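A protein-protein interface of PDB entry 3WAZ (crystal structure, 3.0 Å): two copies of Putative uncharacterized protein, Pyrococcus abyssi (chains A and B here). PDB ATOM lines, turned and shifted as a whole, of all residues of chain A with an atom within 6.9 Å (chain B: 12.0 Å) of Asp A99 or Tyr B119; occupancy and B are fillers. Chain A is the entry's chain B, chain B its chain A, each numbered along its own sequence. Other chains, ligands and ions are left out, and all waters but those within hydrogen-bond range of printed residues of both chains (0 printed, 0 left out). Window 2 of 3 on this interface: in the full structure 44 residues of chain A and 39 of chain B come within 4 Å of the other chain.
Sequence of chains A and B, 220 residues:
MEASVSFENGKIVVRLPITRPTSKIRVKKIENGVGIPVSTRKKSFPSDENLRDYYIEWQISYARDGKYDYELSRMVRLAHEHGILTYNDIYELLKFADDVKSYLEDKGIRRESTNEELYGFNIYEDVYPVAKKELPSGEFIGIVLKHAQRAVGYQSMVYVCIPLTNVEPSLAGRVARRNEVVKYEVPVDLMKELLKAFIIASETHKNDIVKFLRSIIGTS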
ATOM      1  N   LEU A  94      11.640  -5.998  23.392  1.00  0.00           N
ATOM      2  CA  LEU A  94      12.013  -5.979  24.802  1.00  0.00           C
ATOM      3  C   LEU A  94      11.388  -7.152  25.550  1.00  0.00           C
ATOM      4  O   LEU A  94      12.013  -7.741  26.431  1.00  0.00           O
ATOM      5  CB  LEU A  94      11.611  -4.653  25.449  1.00  0.00           C
ATOM      6  CG  LEU A  94      12.379  -3.419  24.969  1.00  0.00           C
ATOM      7  CD1 LEU A  94      11.778  -2.149  25.543  1.00  0.00           C
ATOM      8  CD2 LEU A  94      13.850  -3.529  25.333  1.00  0.00           C
ATOM      9  N   LYS A  95      10.151  -7.487  25.193  1.00  0.00           N
ATOM     10  CA  LYS A  95       9.473  -8.639  25.772  1.00  0.00           C
ATOM     11  C   LYS A  95      10.194  -9.918  25.366  1.00  0.00           C
ATOM     12  O   LYS A  95      10.319 -10.853  26.156  1.00  0.00           O
ATOM     13  CB  LYS A  95       8.017  -8.694  25.309  1.00  0.00           C
ATOM     14  CG  LYS A  95       7.251  -9.897  25.826  1.00  0.00           C
ATOM     15  CD  LYS A  95       5.921 -10.056  25.112  1.00  0.00           C
ATOM     16  CE  LYS A  95       5.179 -11.284  25.614  1.00  0.00           C
ATOM     17  NZ  LYS A  95       5.991 -12.523  25.458  1.00  0.00           N
ATOM     18  N   PHE A  96      10.668  -9.947  24.125  1.00  0.00           N
ATOM     19  CA  PHE A  96      11.408 -11.089  23.603  1.00  0.00           C
ATOM     20  C   PHE A  96      12.718 -11.292  24.356  1.00  0.00           C
ATOM     21  O   PHE A  96      13.093 -12.420  24.674  1.00  0.00           O
ATOM     22  CB  PHE A  96      11.681 -10.904  22.110  1.00  0.00           C
ATOM     23  CG  PHE A  96      12.617 -11.926  21.531  1.00  0.00           C
ATOM     24  CD1 PHE A  96      12.163 -13.190  21.199  1.00  0.00           C
ATOM     25  CD2 PHE A  96      13.948 -11.617  21.306  1.00  0.00           C
ATOM     26  CE1 PHE A  96      13.019 -14.130  20.662  1.00  0.00           C
ATOM     27  CE2 PHE A  96      14.810 -12.554  20.770  1.00  0.00           C
ATOM     28  CZ  PHE A  96      14.345 -13.811  20.446  1.00  0.00           C
ATOM     29  N   ALA A  97      13.409 -10.190  24.634  1.00  0.00           N
ATOM     30  CA  ALA A  97      14.674 -10.231  25.356  1.00  0.00           C
ATOM     31  C   ALA A  97      14.482 -10.737  26.781  1.00  0.00           C
ATOM     32  O   ALA A  97      15.364 -11.384  27.346  1.00  0.00           O
ATOM     33  CB  ALA A  97      15.317  -8.853  25.366  1.00  0.00           C
ATOM     34  N   ASP A  98      13.323 -10.437  27.354  1.00  0.00           N
ATOM     35  CA  ASP A  98      13.020 -10.826  28.725  1.00  0.00           C
ATOM     36  C   ASP A  98      12.802 -12.332  28.839  1.00  0.00           C
ATOM     37  O   ASP A  98      12.914 -12.903  29.922  1.00  0.00           O
ATOM     38  CB  ASP A  98      11.785 -10.075  29.225  1.00  0.00           C
ATOM     39  CG  ASP A  98      11.562 -10.246  30.712  1.00  0.00           C
ATOM     40  OD1 ASP A  98      12.153  -9.472  31.494  1.00  0.00           O
ATOM     41  OD2 ASP A  98      10.797 -11.154  31.100  1.00  0.00           O
ATOM     42  N   ASP A  99      12.496 -12.969  27.713  1.00  0.00           N
ATOM     43  CA  ASP A  99      12.209 -14.400  27.697  1.00  0.00           C
ATOM     44  C   ASP A  99      13.428 -15.237  27.317  1.00  0.00           C
ATOM     45  O   ASP A  99      13.338 -16.459  27.208  1.00  0.00           O
ATOM     46  CB  ASP A  99      11.054 -14.704  26.739  1.00  0.00           C
ATOM     47  CG  ASP A  99       9.766 -14.013  27.142  1.00  0.00           C
ATOM     48  OD1 ASP A  99       9.602 -13.714  28.344  1.00  0.00           O
ATOM     49  OD2 ASP A  99       8.916 -13.771  26.259  1.00  0.00           O
ATOM     50  N   VAL A 100      14.564 -14.578  27.117  1.00  0.00           N
ATOM     51  CA  VAL A 100      15.784 -15.277  26.725  1.00  0.00           C
ATOM     52  C   VAL A 100      16.626 -15.673  27.934  1.00  0.00           C
ATOM     53  O   VAL A 100      17.111 -14.816  28.672  1.00  0.00           O
ATOM     54  CB  VAL A 100      16.633 -14.428  25.762  1.00  0.00           C
ATOM     55  CG1 VAL A 100      17.961 -15.109  25.486  1.00  0.00           C
ATOM     56  CG2 VAL A 100      15.875 -14.183  24.466  1.00  0.00           C
ATOM     57  N   LYS A 101      16.797 -16.977  28.127  1.00  0.00           N
ATOM     58  CA  LYS A 101      17.563 -17.492  29.258  1.00  0.00           C
ATOM     59  C   LYS A 101      18.861 -18.153  28.807  1.00  0.00           C
ATOM     60  O   LYS A 101      19.780 -18.343  29.602  1.00  0.00           O
ATOM     61  CB  LYS A 101      16.733 -18.487  30.077  1.00  0.00           C
ATOM     62  CG  LYS A 101      15.643 -17.858  30.933  1.00  0.00           C
ATOM     63  CD  LYS A 101      14.374 -17.604  30.140  1.00  0.00           C
ATOM     64  CE  LYS A 101      13.286 -17.014  31.020  1.00  0.00           C
ATOM     65  NZ  LYS A 101      12.009 -16.828  30.275  1.00  0.00           N
ATOM     66  N   SER A 102      18.927 -18.509  27.528  1.00  0.00           N
ATOM     67  CA  SER A 102      20.114 -19.149  26.977  1.00  0.00           C
ATOM     68  C   SER A 102      20.598 -18.398  25.740  1.00  0.00           C
ATOM     69  O   SER A 102      19.807 -17.769  25.039  1.00  0.00           O
ATOM     70  CB  SER A 102      19.823 -20.613  26.634  1.00  0.00           C
ATOM     71  OG  SER A 102      21.007 -21.295  26.263  1.00  0.00           O
ATOM     72  N   TYR A 103      21.897 -18.468  25.478  1.00  0.00           N
ATOM     73  CA  TYR A 103      22.489 -17.741  24.360  1.00  0.00           C
ATOM     74  C   TYR A 103      23.329 -18.677  23.500  1.00  0.00           C
ATOM     75  O   TYR A 103      23.663 -19.782  23.926  1.00  0.00           O
ATOM     76  CB  TYR A 103      23.340 -16.579  24.879  1.00  0.00           C
ATOM     77  CG  TYR A 103      22.652 -15.755  25.947  1.00  0.00           C
ATOM     78  CD1 TYR A 103      21.851 -14.672  25.611  1.00  0.00           C
ATOM     79  CD2 TYR A 103      22.801 -16.066  27.293  1.00  0.00           C
ATOM     80  CE1 TYR A 103      21.219 -13.920  26.585  1.00  0.00           C
ATOM     81  CE2 TYR A 103      22.174 -15.322  28.272  1.00  0.00           C
ATOM     82  CZ  TYR A 103      21.384 -14.251  27.914  1.00  0.00           C
ATOM     83  OH  TYR A 103      20.762 -13.511  28.892  1.00  0.00           O
ATOM     84  N   LYS A 133      19.210 -17.172  10.463  1.00  0.00           N
ATOM     85  CA  LYS A 133      17.826 -16.812  10.177  1.00  0.00           C
ATOM     86  C   LYS A 133      17.736 -16.147   8.810  1.00  0.00           C
ATOM     87  O   LYS A 133      18.415 -15.155   8.546  1.00  0.00           O
ATOM     88  CB  LYS A 133      17.277 -15.884  11.259  1.00  0.00           C
ATOM     89  CG  LYS A 133      15.765 -15.766  11.253  1.00  0.00           C
ATOM     90  CD  LYS A 133      15.249 -15.308  12.603  1.00  0.00           C
ATOM     91  CE  LYS A 133      13.747 -15.511  12.712  1.00  0.00           C
ATOM     92  NZ  LYS A 133      13.247 -15.212  14.083  1.00  0.00           N
ATOM     93  N   GLU A 193      15.030  -8.397  13.152  1.00  0.00           N
ATOM     94  CA  GLU A 193      15.668  -9.692  13.365  1.00  0.00           C
ATOM     95  C   GLU A 193      17.140  -9.545  13.734  1.00  0.00           C
ATOM     96  O   GLU A 193      17.713 -10.418  14.386  1.00  0.00           O
ATOM     97  CB  GLU A 193      15.516 -10.588  12.133  1.00  0.00           C
ATOM     98  CG  GLU A 193      14.084 -11.016  11.839  1.00  0.00           C
ATOM     99  CD  GLU A 193      13.495 -11.905  12.920  1.00  0.00           C
ATOM    100  OE1 GLU A 193      14.264 -12.455  13.736  1.00  0.00           O
ATOM    101  OE2 GLU A 193      12.255 -12.054  12.953  1.00  0.00           O
ATOM    102  N   LYS A 196      17.208  -9.064  17.473  1.00  0.00           N
ATOM    103  CA  LYS A 196      16.982 -10.354  18.118  1.00  0.00           C
ATOM    104  C   LYS A 196      18.263 -11.177  18.136  1.00  0.00           C
ATOM    105  O   LYS A 196      18.556 -11.870  19.111  1.00  0.00           O
ATOM    106  CB  LYS A 196      15.898 -11.146  17.386  1.00  0.00           C
ATOM    107  CG  LYS A 196      14.496 -10.586  17.506  1.00  0.00           C
ATOM    108  CD  LYS A 196      13.501 -11.540  16.860  1.00  0.00           C
ATOM    109  CE  LYS A 196      12.114 -10.935  16.769  1.00  0.00           C
ATOM    110  NZ  LYS A 196      11.179 -11.838  16.041  1.00  0.00           N
ATOM    111  N   ILE A 200      20.167 -12.737  21.489  1.00  0.00           N
ATOM    112  CA  ILE A 200      20.439 -14.145  21.774  1.00  0.00           C
ATOM    113  C   ILE A 200      21.908 -14.521  21.571  1.00  0.00           C
ATOM    114  O   ILE A 200      22.312 -15.644  21.871  1.00  0.00           O
ATOM    115  CB  ILE A 200      19.571 -15.075  20.909  1.00  0.00           C
ATOM    116  CG1 ILE A 200      20.083 -15.092  19.468  1.00  0.00           C
ATOM    117  CG2 ILE A 200      18.114 -14.644  20.967  1.00  0.00           C
ATOM    118  CD1 ILE A 200      19.408 -16.128  18.599  1.00  0.00           C
ATOM    119  N   LYS A 206      22.733  -8.569  24.903  1.00  0.00           N
ATOM    120  CA  LYS A 206      21.333  -8.333  25.261  1.00  0.00           C
ATOM    121  C   LYS A 206      21.159  -7.079  26.119  1.00  0.00           C
ATOM    122  O   LYS A 206      20.287  -6.254  25.851  1.00  0.00           O
ATOM    123  CB  LYS A 206      20.748  -9.550  25.988  1.00  0.00           C
ATOM    124  CG  LYS A 206      19.226  -9.516  26.137  1.00  0.00           C
ATOM    125  CD  LYS A 206      18.704 -10.782  26.799  1.00  0.00           C
ATOM    126  CE  LYS A 206      19.129 -10.869  28.257  1.00  0.00           C
ATOM    127  NZ  LYS A 206      18.634 -12.122  28.901  1.00  0.00           N
ATOM    128  N   THR B 114      21.111 -28.778  11.573  1.00  0.00           N
ATOM    129  CA  THR B 114      20.609 -29.607  12.661  1.00  0.00           C
ATOM    130  C   THR B 114      19.106 -29.400  12.787  1.00  0.00           C
ATOM    131  O   THR B 114      18.530 -28.558  12.099  1.00  0.00           O
ATOM    132  CB  THR B 114      21.266 -29.252  14.010  1.00  0.00           C
ATOM    133  OG1 THR B 114      20.780 -27.983  14.466  1.00  0.00           O
ATOM    134  CG2 THR B 114      22.784 -29.197  13.878  1.00  0.00           C
ATOM    135  N   ASN B 115      18.473 -30.168  13.665  1.00  0.00           N
ATOM    136  CA  ASN B 115      17.046 -30.017  13.912  1.00  0.00           C
ATOM    137  C   ASN B 115      16.769 -29.155  15.138  1.00  0.00           C
ATOM    138  O   ASN B 115      15.621 -28.997  15.553  1.00  0.00           O
ATOM    139  CB  ASN B 115      16.375 -31.383  14.057  1.00  0.00           C
ATOM    140  CG  ASN B 115      16.228 -32.103  12.731  1.00  0.00           C
ATOM    141  OD1 ASN B 115      15.858 -31.500  11.724  1.00  0.00           O
ATOM    142  ND2 ASN B 115      16.519 -33.399  12.725  1.00  0.00           N
ATOM    143  N   GLU B 116      17.831 -28.597  15.711  1.00  0.00           N
ATOM    144  CA  GLU B 116      17.707 -27.737  16.881  1.00  0.00           C
ATOM    145  C   GLU B 116      17.401 -26.303  16.470  1.00  0.00           C
ATOM    146  O   GLU B 116      17.816 -25.851  15.404  1.00  0.00           O
ATOM    147  CB  GLU B 116      18.996 -27.759  17.704  1.00  0.00           C
ATOM    148  CG  GLU B 116      19.592 -29.139  17.911  1.00  0.00           C
ATOM    149  CD  GLU B 116      20.809 -29.109  18.815  1.00  0.00           C
ATOM    150  OE1 GLU B 116      21.836 -29.726  18.456  1.00  0.00           O
ATOM    151  OE2 GLU B 116      20.738 -28.472  19.887  1.00  0.00           O
ATOM    152  N   GLU B 117      16.674 -25.592  17.324  1.00  0.00           N
ATOM    153  CA  GLU B 117      16.435 -24.169  17.122  1.00  0.00           C
ATOM    154  C   GLU B 117      16.821 -23.389  18.373  1.00  0.00           C
ATOM    155  O   GLU B 117      17.046 -23.971  19.434  1.00  0.00           O
ATOM    156  CB  GLU B 117      14.973 -23.900  16.764  1.00  0.00           C
ATOM    157  CG  GLU B 117      14.550 -24.441  15.411  1.00  0.00           C
ATOM    158  CD  GLU B 117      13.215 -23.884  14.957  1.00  0.00           C
ATOM    159  OE1 GLU B 117      12.687 -24.360  13.929  1.00  0.00           O
ATOM    160  OE2 GLU B 117      12.697 -22.964  15.626  1.00  0.00           O
ATOM    161  N   LEU B 118      16.903 -22.070  18.238  1.00  0.00           N
ATOM    162  CA  LEU B 118      17.222 -21.206  19.367  1.00  0.00           C
ATOM    163  C   LEU B 118      16.471 -19.885  19.249  1.00  0.00           C
ATOM    164  O   LEU B 118      16.959 -18.940  18.627  1.00  0.00           O
ATOM    165  CB  LEU B 118      18.729 -20.958  19.449  1.00  0.00           C
ATOM    166  CG  LEU B 118      19.221 -20.139  20.645  1.00  0.00           C
ATOM    167  CD1 LEU B 118      18.902 -20.850  21.950  1.00  0.00           C
ATOM    168  CD2 LEU B 118      20.712 -19.861  20.534  1.00  0.00           C
ATOM    169  N   TYR B 119      15.283 -19.838  19.844  1.00  0.00           N
ATOM    170  CA  TYR B 119      14.422 -18.658  19.805  1.00  0.00           C
ATOM    171  C   TYR B 119      14.134 -18.190  18.380  1.00  0.00           C
ATOM    172  O   TYR B 119      14.317 -17.018  18.053  1.00  0.00           O
ATOM    173  CB  TYR B 119      15.020 -17.516  20.631  1.00  0.00           C
ATOM    174  CG  TYR B 119      15.237 -17.867  22.085  1.00  0.00           C
ATOM    175  CD1 TYR B 119      16.490 -18.247  22.548  1.00  0.00           C
ATOM    176  CD2 TYR B 119      14.189 -17.822  22.995  1.00  0.00           C
ATOM    177  CE1 TYR B 119      16.694 -18.571  23.876  1.00  0.00           C
ATOM    178  CE2 TYR B 119      14.382 -18.143  24.325  1.00  0.00           C
ATOM    179  CZ  TYR B 119      15.635 -18.517  24.761  1.00  0.00           C
ATOM    180  OH  TYR B 119      15.830 -18.838  26.084  1.00  0.00           O
ATOM    181  N   GLY B 120      13.683 -19.113  17.536  1.00  0.00           N
ATOM    182  CA  GLY B 120      13.329 -18.786  16.168  1.00  0.00           C
ATOM    183  C   GLY B 120      14.461 -19.005  15.185  1.00  0.00           C
ATOM    184  O   GLY B 120      14.229 -19.279  14.007  1.00  0.00           O
ATOM    185  N   PHE B 121      15.692 -18.883  15.669  1.00  0.00           N
ATOM    186  CA  PHE B 121      16.871 -19.059  14.829  1.00  0.00           C
ATOM    187  C   PHE B 121      17.215 -20.535  14.668  1.00  0.00           C
ATOM    188  O   PHE B 121      17.208 -21.291  15.638  1.00  0.00           O
ATOM    189  CB  PHE B 121      18.067 -18.310  15.422  1.00  0.00           C
ATOM    190  CG  PHE B 121      17.990 -16.816  15.265  1.00  0.00           C
ATOM    191  CD1 PHE B 121      17.052 -16.076  15.965  1.00  0.00           C
ATOM    192  CD2 PHE B 121      18.871 -16.151  14.429  1.00  0.00           C
ATOM    193  CE1 PHE B 121      16.986 -14.703  15.825  1.00  0.00           C
ATOM    194  CE2 PHE B 121      18.811 -14.778  14.285  1.00  0.00           C
ATOM    195  CZ  PHE B 121      17.866 -14.054  14.983  1.00  0.00           C
ATOM    196  N   ASN B 122      17.516 -20.940  13.438  1.00  0.00           N
ATOM    197  CA  ASN B 122      17.927 -22.314  13.170  1.00  0.00           C
ATOM    198  C   ASN B 122      19.394 -22.540  13.514  1.00  0.00           C
ATOM    199  O   ASN B 122      20.234 -21.669  13.291  1.00  0.00           O
ATOM    200  CB  ASN B 122      17.661 -22.686  11.711  1.00  0.00           C
ATOM    201  CG  ASN B 122      16.185 -22.839  11.411  1.00  0.00           C
ATOM    202  OD1 ASN B 122      15.620 -23.923  11.558  1.00  0.00           O
ATOM    203  ND2 ASN B 122      15.550 -21.752  10.989  1.00  0.00           N
ATOM    204  N   ILE B 123      19.693 -23.713  14.059  1.00  0.00           N
ATOM    205  CA  ILE B 123      21.052 -24.038  14.476  1.00  0.00           C
ATOM    206  C   ILE B 123      21.823 -24.797  13.402  1.00  0.00           C
ATOM    207  O   ILE B 123      21.358 -25.814  12.885  1.00  0.00           O
ATOM    208  CB  ILE B 123      21.059 -24.855  15.784  1.00  0.00           C
ATOM    209  CG1 ILE B 123      20.520 -24.009  16.937  1.00  0.00           C
ATOM    210  CG2 ILE B 123      22.464 -25.346  16.103  1.00  0.00           C
ATOM    211  CD1 ILE B 123      21.308 -22.741  17.179  1.00  0.00           C
ATOM    212  N   TYR B 124      23.005 -24.289  13.070  1.00  0.00           N
ATOM    213  CA  TYR B 124      23.891 -24.950  12.121  1.00  0.00           C
ATOM    214  C   TYR B 124      25.239 -25.238  12.765  1.00  0.00           C
ATOM    215  O   TYR B 124      25.502 -24.819  13.893  1.00  0.00           O
ATOM    216  CB  TYR B 124      24.089 -24.088  10.875  1.00  0.00           C
ATOM    217  CG  TYR B 124      22.860 -23.966  10.008  1.00  0.00           C
ATOM    218  CD1 TYR B 124      21.888 -23.013  10.278  1.00  0.00           C
ATOM    219  CD2 TYR B 124      22.674 -24.800   8.913  1.00  0.00           C
ATOM    220  CE1 TYR B 124      20.762 -22.897   9.486  1.00  0.00           C
ATOM    221  CE2 TYR B 124      21.551 -24.692   8.116  1.00  0.00           C
ATOM    222  CZ  TYR B 124      20.599 -23.739   8.407  1.00  0.00           C
ATOM    223  OH  TYR B 124      19.479 -23.623   7.615  1.00  0.00           O
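OH of Tyr B119 is in hydrogen-bond range of N of Lys A101 (2.9 Å).
OH of Tyr B119 sits at hydrogen-bond distance from N of Ser A102 (3.4 Å).
The side-chain amino group of Lys A95 lies within salt-bridge range of the side-chain carboxylate of Asp A99.
The side-chain amino group (NZ) of Lys A101 lies close to the backbone carbonyl oxygen (O) of Asp A99, 3.4 Å away.
The side-chain carboxylate (OE1) of Glu A193 is in salt-bridge range of the side-chain amino group (NZ) of Lys A133, at 3.0 Å.
The side-chain amino group (NZ) of Lys A196 lies within salt-bridge range of the side-chain carboxylate (OE2) of Glu A193, 3.3 Å away.
O of Val A100 is in hydrogen-bond range of NZ of Lys A206.
Phe A96 touches Tyr B119 (CZ to CB, 3.8 Å).
O of Asp A99 touches CE2 of Tyr B119, 3.5 Å away.
Val A100 touches Tyr B119.
CB of Lys A133 touches CD2 of Phe B121, at 3.6 Å.
O of Glu A193 touches CZ of Phe B121, at 3.7 Å.
Leu B118 touches Ile A200 (O to CD1, 3.7 Å).
Ile A200 touches Phe B121.
Asp A99 touches just one residue of chain B: Tyr B119.
Tyr B119 touches just these residues of chain A: Phe A96, Asp A99, Val A100, Lys A101 and Ser A102.
No residue of chain B comes within 4 Å of Lys A95.
Phe A96 touches just one residue of chain B: Tyr B119 (3.8 Å).
Ala A97 touches none of the printed residues of chain B.
No residue of chain B comes within 4 Å of Asp A98.
Of the printed residues of chain B, Val A100 touches Tyr B119 (3.6 Å).
Of chain B, only Tyr B119 (2.9 Å) comes within 4 Å of Lys A101.
Ser A102 touches just one residue of chain B: Tyr B119.
Tyr A103 touches none of the printed residues of chain B.
Of chain B, only Leu B118 (3.7 Å) and Phe B121 (3.5 Å) come within 4 Å of Ile A200.
Of the printed residues of chain A, Leu B118 touches Ile A200.
Of the printed residues of chain B, Glu A193 touches Phe B121 (3.7 Å).
Thr B114 touches none of the printed residues of chain A.
Of the 11 printed residues of chain B, 3 touch a printed residue of chain A.
Printed residues of chain A that touch a printed residue of chain B: Phe A96, Asp A99, Val A100, Lys A101, Ser A102, Lys A133, Glu A193 and Ile A200.
Hydrophobic or aromatic side chains of chain A within 4 Å of the printed part of chain B: Phe A96 and Ile A200.
Along chain A the printed residues that touch a printed residue of chain B span positions 96 to 200.
No position is printed for both chains.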
